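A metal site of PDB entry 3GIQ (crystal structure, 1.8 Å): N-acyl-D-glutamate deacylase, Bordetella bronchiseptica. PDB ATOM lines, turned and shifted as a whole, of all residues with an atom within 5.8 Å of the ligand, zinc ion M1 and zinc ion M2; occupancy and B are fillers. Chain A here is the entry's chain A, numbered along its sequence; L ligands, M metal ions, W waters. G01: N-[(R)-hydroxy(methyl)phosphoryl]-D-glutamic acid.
Zinc ion M1 is bound by ND1 of His 218 (2.0 Å), OPB of the ligand (2.0 Å), NE2 of His 248 (2.2 Å) and SG of Cys 95 (2.3 Å). Zinc ion M1 has four donor atoms within binding distance.
Zinc ion M2 is bound by NE2 of His 68 (2.0 Å), OPA of the ligand (2.0 Å), NE2 of His 66 (2.1 Å) and SG of Cys 95 (2.4 Å). Zinc ion M2 has four donor atoms within binding distance.
Three residues have an atom within 4 Å of zinc ion M1: Cys 95, His 218 and His 248.
NH1 of Arg 376 is in salt-bridge range of O of the ligand (2.7 Å). OPA of the ligand lies close to OD2 of Asp 365. An oxygen (OXT) of the ligand lies within salt-bridge range of the side-chain amino group (NZ) of Lys 250 (2.8 Å). OG of Ser 287 sits at hydrogen-bond distance from OE1 of the ligand, at 2.7 Å. The side-chain hydroxyl of Tyr 190 sits close to an oxygen (OPB) of the ligand, at 2.7 Å. An oxygen (OE2) of the ligand lies within salt-bridge range of the guanidinium group (NH2) of Arg 295, at 2.7 Å. An oxygen (O) of the ligand is in hydrogen-bond range of the backbone NH of Ser 288, 2.8 Å away. OH of Tyr 282 is in hydrogen-bond range of OXT of the ligand, 2.7 Å away. The backbone carbonyl oxygen of Ser 288 sits at hydrogen-bond distance from a nitrogen (N) of the ligand (2.8 Å).
OH of Tyr 282 lies close to NH1 of Arg 376, at 3.4 Å. NH2 of Arg 376 sits at hydrogen-bond distance from O of Ser 288 (3.0 Å). A ring nitrogen (ND1) of His 248 is in hydrogen-bond range of the side-chain carboxylate (OE2) of Glu 222, 3.1 Å away. O of Glu 222 lies within hydrogen-bond range of N of Met 252 (2.8 Å). The backbone NH (N) of Asp 365 is in hydrogen-bond range of the backbone carbonyl oxygen (O) of His 66, 2.9 Å away. NZ of Lys 250 lies within salt-bridge range of OE1 of Glu 222. O of Tyr 343 is in hydrogen-bond range of N of Ser 287 (2.8 Å). O of His 248 sits at hydrogen-bond distance from NZ of Lys 250, 2.8 Å away.
Merely in contact with zinc ion M2: Asp 365. Within 4 Å of zinc ion M2: His 66, His 68, Cys 95 and Asp 365. The nearest printed residue that does not touch zinc ion M2 is His 248 (4.03 Å).
Water W1 lies within hydrogen-bond range of OE2 of the ligand (2.6 Å), OE1 of Glu 222 (2.7 Å) and NE2 of His 218 (2.8 Å).
An oxygen (OE1) of the ligand lies close to the side-chain sulfur of Met 252 (3.7 Å). Residues that only touch the ligand: Glu 222, Thr 289, Leu 114 and Tyr 343. Of the 26 residues printed, 18 come within 4 Å of the ligand. The nearest printed residue that does not touch the ligand is Leu 367 (4.2 Å).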
ATOM      1  N   HIS A  66     -10.691   7.142  11.658  1.00  0.00           N
ATOM      2  CA  HIS A  66     -11.933   6.400  11.796  1.00  0.00           C
ATOM      3  C   HIS A  66     -12.618   6.660  13.132  1.00  0.00           C
ATOM      4  O   HIS A  66     -12.587   5.827  14.038  1.00  0.00           O
ATOM      5  CB  HIS A  66     -11.704   4.893  11.638  1.00  0.00           C
ATOM      6  CG  HIS A  66     -12.962   4.142  11.325  1.00  0.00           C
ATOM      7  ND1 HIS A  66     -13.328   3.824  10.029  1.00  0.00           N
ATOM      8  CD2 HIS A  66     -13.980   3.728  12.116  1.00  0.00           C
ATOM      9  CE1 HIS A  66     -14.519   3.237  10.045  1.00  0.00           C
ATOM     10  NE2 HIS A  66     -14.930   3.172  11.301  1.00  0.00           N
ATOM     11  N   GLY A  67     -13.225   7.829  13.244  1.00  0.00           N
ATOM     12  CA  GLY A  67     -13.921   8.169  14.472  1.00  0.00           C
ATOM     13  C   GLY A  67     -15.435   8.094  14.320  1.00  0.00           C
ATOM     14  O   GLY A  67     -15.968   8.160  13.205  1.00  0.00           O
ATOM     15  N   HIS A  68     -16.110   7.919  15.450  1.00  0.00           N
ATOM     16  CA  HIS A  68     -17.571   7.878  15.496  1.00  0.00           C
ATOM     17  C   HIS A  68     -17.985   8.845  16.607  1.00  0.00           C
ATOM     18  O   HIS A  68     -19.012   8.656  17.266  1.00  0.00           O
ATOM     19  CB  HIS A  68     -18.065   6.459  15.815  1.00  0.00           C
ATOM     20  CG  HIS A  68     -18.056   5.535  14.638  1.00  0.00           C
ATOM     21  ND1 HIS A  68     -18.774   5.774  13.490  1.00  0.00           N
ATOM     22  CD2 HIS A  68     -17.383   4.373  14.424  1.00  0.00           C
ATOM     23  CE1 HIS A  68     -18.553   4.802  12.624  1.00  0.00           C
ATOM     24  NE2 HIS A  68     -17.710   3.944  13.159  1.00  0.00           N
ATOM     25  N   ASN A  94     -18.227   8.021   9.862  1.00  0.00           N
ATOM     26  CA  ASN A  94     -17.821   6.789   9.198  1.00  0.00           C
ATOM     27  C   ASN A  94     -18.867   5.674   9.134  1.00  0.00           C
ATOM     28  O   ASN A  94     -19.893   5.726   9.809  1.00  0.00           O
ATOM     29  CB  ASN A  94     -16.554   6.240   9.882  1.00  0.00           C
ATOM     30  CG  ASN A  94     -15.317   7.036   9.519  1.00  0.00           C
ATOM     31  OD1 ASN A  94     -14.798   6.907   8.414  1.00  0.00           O
ATOM     32  ND2 ASN A  94     -14.847   7.871  10.433  1.00  0.00           N
ATOM     33  N   CYS A  95     -18.587   4.672   8.313  1.00  0.00           N
ATOM     34  CA  CYS A  95     -19.445   3.502   8.150  1.00  0.00           C
ATOM     35  C   CYS A  95     -20.907   3.774   7.791  1.00  0.00           C
ATOM     36  O   CYS A  95     -21.801   3.023   8.191  1.00  0.00           O
ATOM     37  CB  CYS A  95     -19.371   2.656   9.420  1.00  0.00           C
ATOM     38  SG  CYS A  95     -17.666   2.196   9.813  1.00  0.00           S
ATOM     39  N   LEU A 114     -25.220   4.135  17.702  1.00  0.00           N
ATOM     40  CA  LEU A 114     -23.841   4.146  18.184  1.00  0.00           C
ATOM     41  C   LEU A 114     -23.248   5.547  18.305  1.00  0.00           C
ATOM     42  O   LEU A 114     -22.280   5.749  19.041  1.00  0.00           O
ATOM     43  CB  LEU A 114     -22.953   3.304  17.265  1.00  0.00           C
ATOM     44  CG  LEU A 114     -23.237   1.802  17.221  1.00  0.00           C
ATOM     45  CD1 LEU A 114     -22.227   1.133  16.276  1.00  0.00           C
ATOM     46  CD2 LEU A 114     -23.126   1.221  18.619  1.00  0.00           C
ATOM     47  N   ALA A 189     -22.514  -3.354   5.017  1.00  0.00           N
ATOM     48  CA  ALA A 189     -22.817  -4.563   5.774  1.00  0.00           C
ATOM     49  C   ALA A 189     -24.021  -4.318   6.679  1.00  0.00           C
ATOM     50  O   ALA A 189     -24.480  -5.218   7.379  1.00  0.00           O
ATOM     51  CB  ALA A 189     -21.605  -4.982   6.606  1.00  0.00           C
ATOM     52  N   TYR A 190     -24.524  -3.081   6.664  1.00  0.00           N
ATOM     53  CA  TYR A 190     -25.656  -2.673   7.500  1.00  0.00           C
ATOM     54  C   TYR A 190     -26.847  -2.160   6.693  1.00  0.00           C
ATOM     55  O   TYR A 190     -26.710  -1.766   5.538  1.00  0.00           O
ATOM     56  CB  TYR A 190     -25.254  -1.519   8.428  1.00  0.00           C
ATOM     57  CG  TYR A 190     -24.064  -1.757   9.326  1.00  0.00           C
ATOM     58  CD1 TYR A 190     -24.081  -2.752  10.300  1.00  0.00           C
ATOM     59  CD2 TYR A 190     -22.939  -0.929   9.253  1.00  0.00           C
ATOM     60  CE1 TYR A 190     -23.023  -2.911  11.192  1.00  0.00           C
ATOM     61  CE2 TYR A 190     -21.873  -1.074  10.139  1.00  0.00           C
ATOM     62  CZ  TYR A 190     -21.927  -2.066  11.109  1.00  0.00           C
ATOM     63  OH  TYR A 190     -20.898  -2.205  12.012  1.00  0.00           O
ATOM     64  N   HIS A 218     -17.199   0.804   4.691  1.00  0.00           N
ATOM     65  CA  HIS A 218     -17.260  -0.354   5.562  1.00  0.00           C
ATOM     66  C   HIS A 218     -17.870  -1.251   4.488  1.00  0.00           C
ATOM     67  O   HIS A 218     -19.051  -1.116   4.150  1.00  0.00           O
ATOM     68  CB  HIS A 218     -18.251  -0.145   6.704  1.00  0.00           C
ATOM     69  CG  HIS A 218     -18.495  -1.385   7.505  1.00  0.00           C
ATOM     70  ND1 HIS A 218     -18.645  -1.366   8.874  1.00  0.00           N
ATOM     71  CD2 HIS A 218     -18.618  -2.674   7.128  1.00  0.00           C
ATOM     72  CE1 HIS A 218     -18.854  -2.599   9.310  1.00  0.00           C
ATOM     73  NE2 HIS A 218     -18.846  -3.412   8.269  1.00  0.00           N
ATOM     74  N   GLU A 222     -17.131  -8.742   5.627  1.00  0.00           N
ATOM     75  CA  GLU A 222     -15.740  -8.862   6.030  1.00  0.00           C
ATOM     76  C   GLU A 222     -15.372 -10.271   6.488  1.00  0.00           C
ATOM     77  O   GLU A 222     -14.387 -10.475   7.186  1.00  0.00           O
ATOM     78  CB  GLU A 222     -15.425  -7.840   7.131  1.00  0.00           C
ATOM     79  CG  GLU A 222     -15.683  -6.409   6.676  1.00  0.00           C
ATOM     80  CD  GLU A 222     -15.217  -5.371   7.666  1.00  0.00           C
ATOM     81  OE1 GLU A 222     -15.772  -5.316   8.783  1.00  0.00           O
ATOM     82  OE2 GLU A 222     -14.283  -4.612   7.337  1.00  0.00           O
ATOM     83  N   SER A 247     -12.312   1.046   5.127  1.00  0.00           N
ATOM     84  CA  SER A 247     -12.352   1.200   6.571  1.00  0.00           C
ATOM     85  C   SER A 247     -12.096  -0.083   7.337  1.00  0.00           C
ATOM     86  O   SER A 247     -12.467  -1.170   6.892  1.00  0.00           O
ATOM     87  CB  SER A 247     -13.722   1.753   7.003  1.00  0.00           C
ATOM     88  OG  SER A 247     -13.985   2.998   6.384  1.00  0.00           O
ATOM     89  N   HIS A 248     -11.456   0.059   8.497  1.00  0.00           N
ATOM     90  CA  HIS A 248     -11.122  -1.064   9.380  1.00  0.00           C
ATOM     91  C   HIS A 248     -11.001  -2.386   8.637  1.00  0.00           C
ATOM     92  O   HIS A 248     -11.730  -3.343   8.908  1.00  0.00           O
ATOM     93  CB  HIS A 248     -12.165  -1.179  10.504  1.00  0.00           C
ATOM     94  CG  HIS A 248     -13.589  -1.165  10.037  1.00  0.00           C
ATOM     95  ND1 HIS A 248     -14.079  -2.040   9.080  1.00  0.00           N
ATOM     96  CD2 HIS A 248     -14.647  -0.413  10.426  1.00  0.00           C
ATOM     97  CE1 HIS A 248     -15.369  -1.822   8.907  1.00  0.00           C
ATOM     98  NE2 HIS A 248     -15.739  -0.845   9.712  1.00  0.00           N
ATOM     99  N   LYS A 250     -10.152  -5.950   7.552  1.00  0.00           N
ATOM    100  CA  LYS A 250      -9.940  -7.148   8.359  1.00  0.00           C
ATOM    101  C   LYS A 250     -10.500  -8.372   7.655  1.00  0.00           C
ATOM    102  O   LYS A 250     -11.152  -8.264   6.613  1.00  0.00           O
ATOM    103  CB  LYS A 250     -10.707  -6.989   9.677  1.00  0.00           C
ATOM    104  CG  LYS A 250     -12.223  -6.976   9.443  1.00  0.00           C
ATOM    105  CD  LYS A 250     -13.042  -6.962  10.732  1.00  0.00           C
ATOM    106  CE  LYS A 250     -13.040  -5.600  11.398  1.00  0.00           C
ATOM    107  NZ  LYS A 250     -13.645  -4.548  10.518  1.00  0.00           N
ATOM    108  N   MET A 252     -12.649 -11.647   9.045  1.00  0.00           N
ATOM    109  CA  MET A 252     -13.316 -12.283  10.173  1.00  0.00           C
ATOM    110  C   MET A 252     -13.609 -13.771   9.964  1.00  0.00           C
ATOM    111  O   MET A 252     -13.948 -14.193   8.857  1.00  0.00           O
ATOM    112  CB  MET A 252     -14.624 -11.557  10.490  1.00  0.00           C
ATOM    113  CG  MET A 252     -14.425 -10.119  10.917  1.00  0.00           C
ATOM    114  SD  MET A 252     -15.990  -9.293  11.263  1.00  0.00           S
ATOM    115  CE  MET A 252     -16.358  -9.985  12.880  1.00  0.00           C
ATOM    116  N   TYR A 282      -7.468  -0.805  13.414  1.00  0.00           N
ATOM    117  CA  TYR A 282      -7.290  -0.510  14.826  1.00  0.00           C
ATOM    118  C   TYR A 282      -6.482  -1.761  15.204  1.00  0.00           C
ATOM    119  O   TYR A 282      -6.710  -2.847  14.656  1.00  0.00           O
ATOM    120  CB  TYR A 282      -8.623  -0.412  15.572  1.00  0.00           C
ATOM    121  CG  TYR A 282      -9.652  -1.460  15.216  1.00  0.00           C
ATOM    122  CD1 TYR A 282      -9.618  -2.728  15.794  1.00  0.00           C
ATOM    123  CD2 TYR A 282     -10.677  -1.160  14.313  1.00  0.00           C
ATOM    124  CE1 TYR A 282     -10.585  -3.681  15.480  1.00  0.00           C
ATOM    125  CE2 TYR A 282     -11.648  -2.105  13.998  1.00  0.00           C
ATOM    126  CZ  TYR A 282     -11.594  -3.359  14.596  1.00  0.00           C
ATOM    127  OH  TYR A 282     -12.557  -4.286  14.296  1.00  0.00           O
ATOM    128  N   GLY A 286     -10.380  -8.068  17.796  1.00  0.00           N
ATOM    129  CA  GLY A 286     -11.790  -8.143  18.109  1.00  0.00           C
ATOM    130  C   GLY A 286     -12.464  -6.906  17.559  1.00  0.00           C
ATOM    131  O   GLY A 286     -11.910  -5.814  17.645  1.00  0.00           O
ATOM    132  N   SER A 287     -13.647  -7.060  16.965  1.00  0.00           N
ATOM    133  CA  SER A 287     -14.365  -5.901  16.423  1.00  0.00           C
ATOM    134  C   SER A 287     -15.432  -5.478  17.428  1.00  0.00           C
ATOM    135  O   SER A 287     -15.555  -6.061  18.491  1.00  0.00           O
ATOM    136  CB  SER A 287     -15.012  -6.256  15.085  1.00  0.00           C
ATOM    137  OG  SER A 287     -16.034  -7.231  15.256  1.00  0.00           O
ATOM    138  N   SER A 288     -16.188  -4.445  17.080  1.00  0.00           N
ATOM    139  CA  SER A 288     -17.256  -3.974  17.968  1.00  0.00           C
ATOM    140  C   SER A 288     -18.260  -3.132  17.203  1.00  0.00           C
ATOM    141  O   SER A 288     -17.907  -2.182  16.506  1.00  0.00           O
ATOM    142  CB  SER A 288     -16.679  -3.171  19.130  1.00  0.00           C
ATOM    143  OG  SER A 288     -17.709  -2.802  20.038  1.00  0.00           O
ATOM    144  N   THR A 289     -19.536  -3.495  17.338  1.00  0.00           N
ATOM    145  CA  THR A 289     -20.614  -2.777  16.677  1.00  0.00           C
ATOM    146  C   THR A 289     -21.916  -3.207  17.350  1.00  0.00           C
ATOM    147  O   THR A 289     -21.889  -3.630  18.506  1.00  0.00           O
ATOM    148  CB  THR A 289     -20.654  -3.097  15.157  1.00  0.00           C
ATOM    149  OG1 THR A 289     -21.646  -2.286  14.515  1.00  0.00           O
ATOM    150  CG2 THR A 289     -20.969  -4.567  14.919  1.00  0.00           C
ATOM    151  N   ILE A 292     -25.532  -8.546  16.854  1.00  0.00           N
ATOM    152  CA  ILE A 292     -26.179  -9.219  15.736  1.00  0.00           C
ATOM    153  C   ILE A 292     -26.494 -10.648  16.138  1.00  0.00           C
ATOM    154  O   ILE A 292     -25.611 -11.502  16.192  1.00  0.00           O
ATOM    155  CB  ILE A 292     -25.244  -9.221  14.507  1.00  0.00           C
ATOM    156  CG1 ILE A 292     -24.925  -7.780  14.106  1.00  0.00           C
ATOM    157  CG2 ILE A 292     -25.888  -9.978  13.352  1.00  0.00           C
ATOM    158  CD1 ILE A 292     -23.769  -7.656  13.106  1.00  0.00           C
ATOM    159  N   ARG A 295     -25.122 -13.966  14.753  1.00  0.00           N
ATOM    160  CA  ARG A 295     -23.742 -14.356  15.060  1.00  0.00           C
ATOM    161  C   ARG A 295     -23.616 -15.147  16.365  1.00  0.00           C
ATOM    162  O   ARG A 295     -22.549 -15.663  16.676  1.00  0.00           O
ATOM    163  CB  ARG A 295     -22.852 -13.111  15.164  1.00  0.00           C
ATOM    164  CG  ARG A 295     -22.690 -12.352  13.868  1.00  0.00           C
ATOM    165  CD  ARG A 295     -21.766 -11.154  14.070  1.00  0.00           C
ATOM    166  NE  ARG A 295     -21.469 -10.466  12.814  1.00  0.00           N
ATOM    167  CZ  ARG A 295     -20.640  -9.444  12.707  1.00  0.00           C
ATOM    168  NH1 ARG A 295     -20.018  -8.971  13.782  1.00  0.00           N
ATOM    169  NH2 ARG A 295     -20.408  -8.892  11.525  1.00  0.00           N
ATOM    170  N   TYR A 343     -16.717  -8.674  19.113  1.00  0.00           N
ATOM    171  CA  TYR A 343     -16.587  -9.967  18.452  1.00  0.00           C
ATOM    172  C   TYR A 343     -15.121 -10.323  18.244  1.00  0.00           C
ATOM    173  O   TYR A 343     -14.433  -9.669  17.461  1.00  0.00           O
ATOM    174  CB  TYR A 343     -17.294  -9.903  17.091  1.00  0.00           C
ATOM    175  CG  TYR A 343     -18.748  -9.460  17.158  1.00  0.00           C
ATOM    176  CD1 TYR A 343     -19.770 -10.367  17.409  1.00  0.00           C
ATOM    177  CD2 TYR A 343     -19.094  -8.118  16.932  1.00  0.00           C
ATOM    178  CE1 TYR A 343     -21.108  -9.972  17.444  1.00  0.00           C
ATOM    179  CE2 TYR A 343     -20.441  -7.704  16.965  1.00  0.00           C
ATOM    180  CZ  TYR A 343     -21.437  -8.642  17.225  1.00  0.00           C
ATOM    181  OH  TYR A 343     -22.758  -8.267  17.223  1.00  0.00           O
ATOM    182  N   MET A 346     -10.818 -12.147  14.623  1.00  0.00           N
ATOM    183  CA  MET A 346      -9.705 -11.917  13.719  1.00  0.00           C
ATOM    184  C   MET A 346      -8.403 -12.533  14.219  1.00  0.00           C
ATOM    185  O   MET A 346      -8.280 -12.893  15.386  1.00  0.00           O
ATOM    186  CB  MET A 346      -9.502 -10.419  13.480  1.00  0.00           C
ATOM    187  CG  MET A 346     -10.662  -9.730  12.761  1.00  0.00           C
ATOM    188  SD  MET A 346     -11.867  -8.978  13.869  1.00  0.00           S
ATOM    189  CE  MET A 346     -11.066  -7.424  14.215  1.00  0.00           C
ATOM    190  N   ASP A 365     -11.649   3.724  15.762  1.00  0.00           N
ATOM    191  CA  ASP A 365     -13.005   3.183  15.670  1.00  0.00           C
ATOM    192  C   ASP A 365     -13.628   3.098  17.065  1.00  0.00           C
ATOM    193  O   ASP A 365     -14.403   2.191  17.374  1.00  0.00           O
ATOM    194  CB  ASP A 365     -13.001   1.813  15.005  1.00  0.00           C
ATOM    195  CG  ASP A 365     -14.362   1.444  14.422  1.00  0.00           C
ATOM    196  OD1 ASP A 365     -15.279   2.293  14.452  1.00  0.00           O
ATOM    197  OD2 ASP A 365     -14.520   0.301  13.932  1.00  0.00           O
ATOM    198  N   LEU A 367     -16.063   3.698  20.127  1.00  0.00           N
ATOM    199  CA  LEU A 367     -17.508   3.889  20.225  1.00  0.00           C
ATOM    200  C   LEU A 367     -17.699   4.523  21.603  1.00  0.00           C
ATOM    201  O   LEU A 367     -17.992   3.842  22.590  1.00  0.00           O
ATOM    202  CB  LEU A 367     -18.218   2.544  20.124  1.00  0.00           C
ATOM    203  CG  LEU A 367     -17.944   1.813  18.796  1.00  0.00           C
ATOM    204  CD1 LEU A 367     -18.698   0.500  18.754  1.00  0.00           C
ATOM    205  CD2 LEU A 367     -18.348   2.698  17.631  1.00  0.00           C
ATOM    206  N   ARG A 376     -10.115  -0.057  22.257  1.00  0.00           N
ATOM    207  CA  ARG A 376      -9.540   0.730  21.165  1.00  0.00           C
ATOM    208  C   ARG A 376      -9.931   2.195  21.297  1.00  0.00           C
ATOM    209  O   ARG A 376      -9.263   3.080  20.758  1.00  0.00           O
ATOM    210  CB  ARG A 376     -10.023   0.186  19.818  1.00  0.00           C
ATOM    211  CG  ARG A 376     -11.507   0.372  19.565  1.00  0.00           C
ATOM    212  CD  ARG A 376     -11.966  -0.484  18.404  1.00  0.00           C
ATOM    213  NE  ARG A 376     -13.365  -0.237  18.048  1.00  0.00           N
ATOM    214  CZ  ARG A 376     -14.083  -1.021  17.262  1.00  0.00           C
ATOM    215  NH1 ARG A 376     -13.548  -2.127  16.756  1.00  0.00           N
ATOM    216  NH2 ARG A 376     -15.336  -0.711  16.970  1.00  0.00           N
HETATM  217  CD  G01 L   1     -18.091  -6.407  12.345  1.00  0.00           C
HETATM  218  CG  G01 L   1     -17.162  -5.207  12.171  1.00  0.00           C
HETATM  219  CB  G01 L   1     -17.662  -4.032  13.009  1.00  0.00           C
HETATM  220  CA  G01 L   1     -16.848  -2.701  13.034  1.00  0.00           C
HETATM  221  C   G01 L   1     -15.453  -2.981  13.635  1.00  0.00           C
HETATM  222  C6  G01 L   1     -19.231   0.514  14.095  1.00  0.00           C
HETATM  223  P   G01 L   1     -18.068  -0.281  12.999  1.00  0.00           P
HETATM  224  OPA G01 L   1     -16.852   0.722  12.801  1.00  0.00           O
HETATM  225  OPB G01 L   1     -18.738  -0.563  11.699  1.00  0.00           O
HETATM  226  N   G01 L   1     -17.500  -1.583  13.785  1.00  0.00           N
HETATM  227  O   G01 L   1     -15.306  -2.922  14.869  1.00  0.00           O
HETATM  228  OXT G01 L   1     -14.552  -3.244  12.821  1.00  0.00           O
HETATM  229  OE1 G01 L   1     -17.999  -7.047  13.418  1.00  0.00           O
HETATM  230  OE2 G01 L   1     -18.880  -6.637  11.411  1.00  0.00           O
HETATM  231 ZN    ZN M   1     -17.751  -0.080  10.055  1.00  0.00          ZN
HETATM  232 ZN    ZN M   2     -16.803   2.574  12.054  1.00  0.00          ZN
HETATM  233  O   HOH W   1     -18.346  -6.077   8.902  1.00  0.00           O
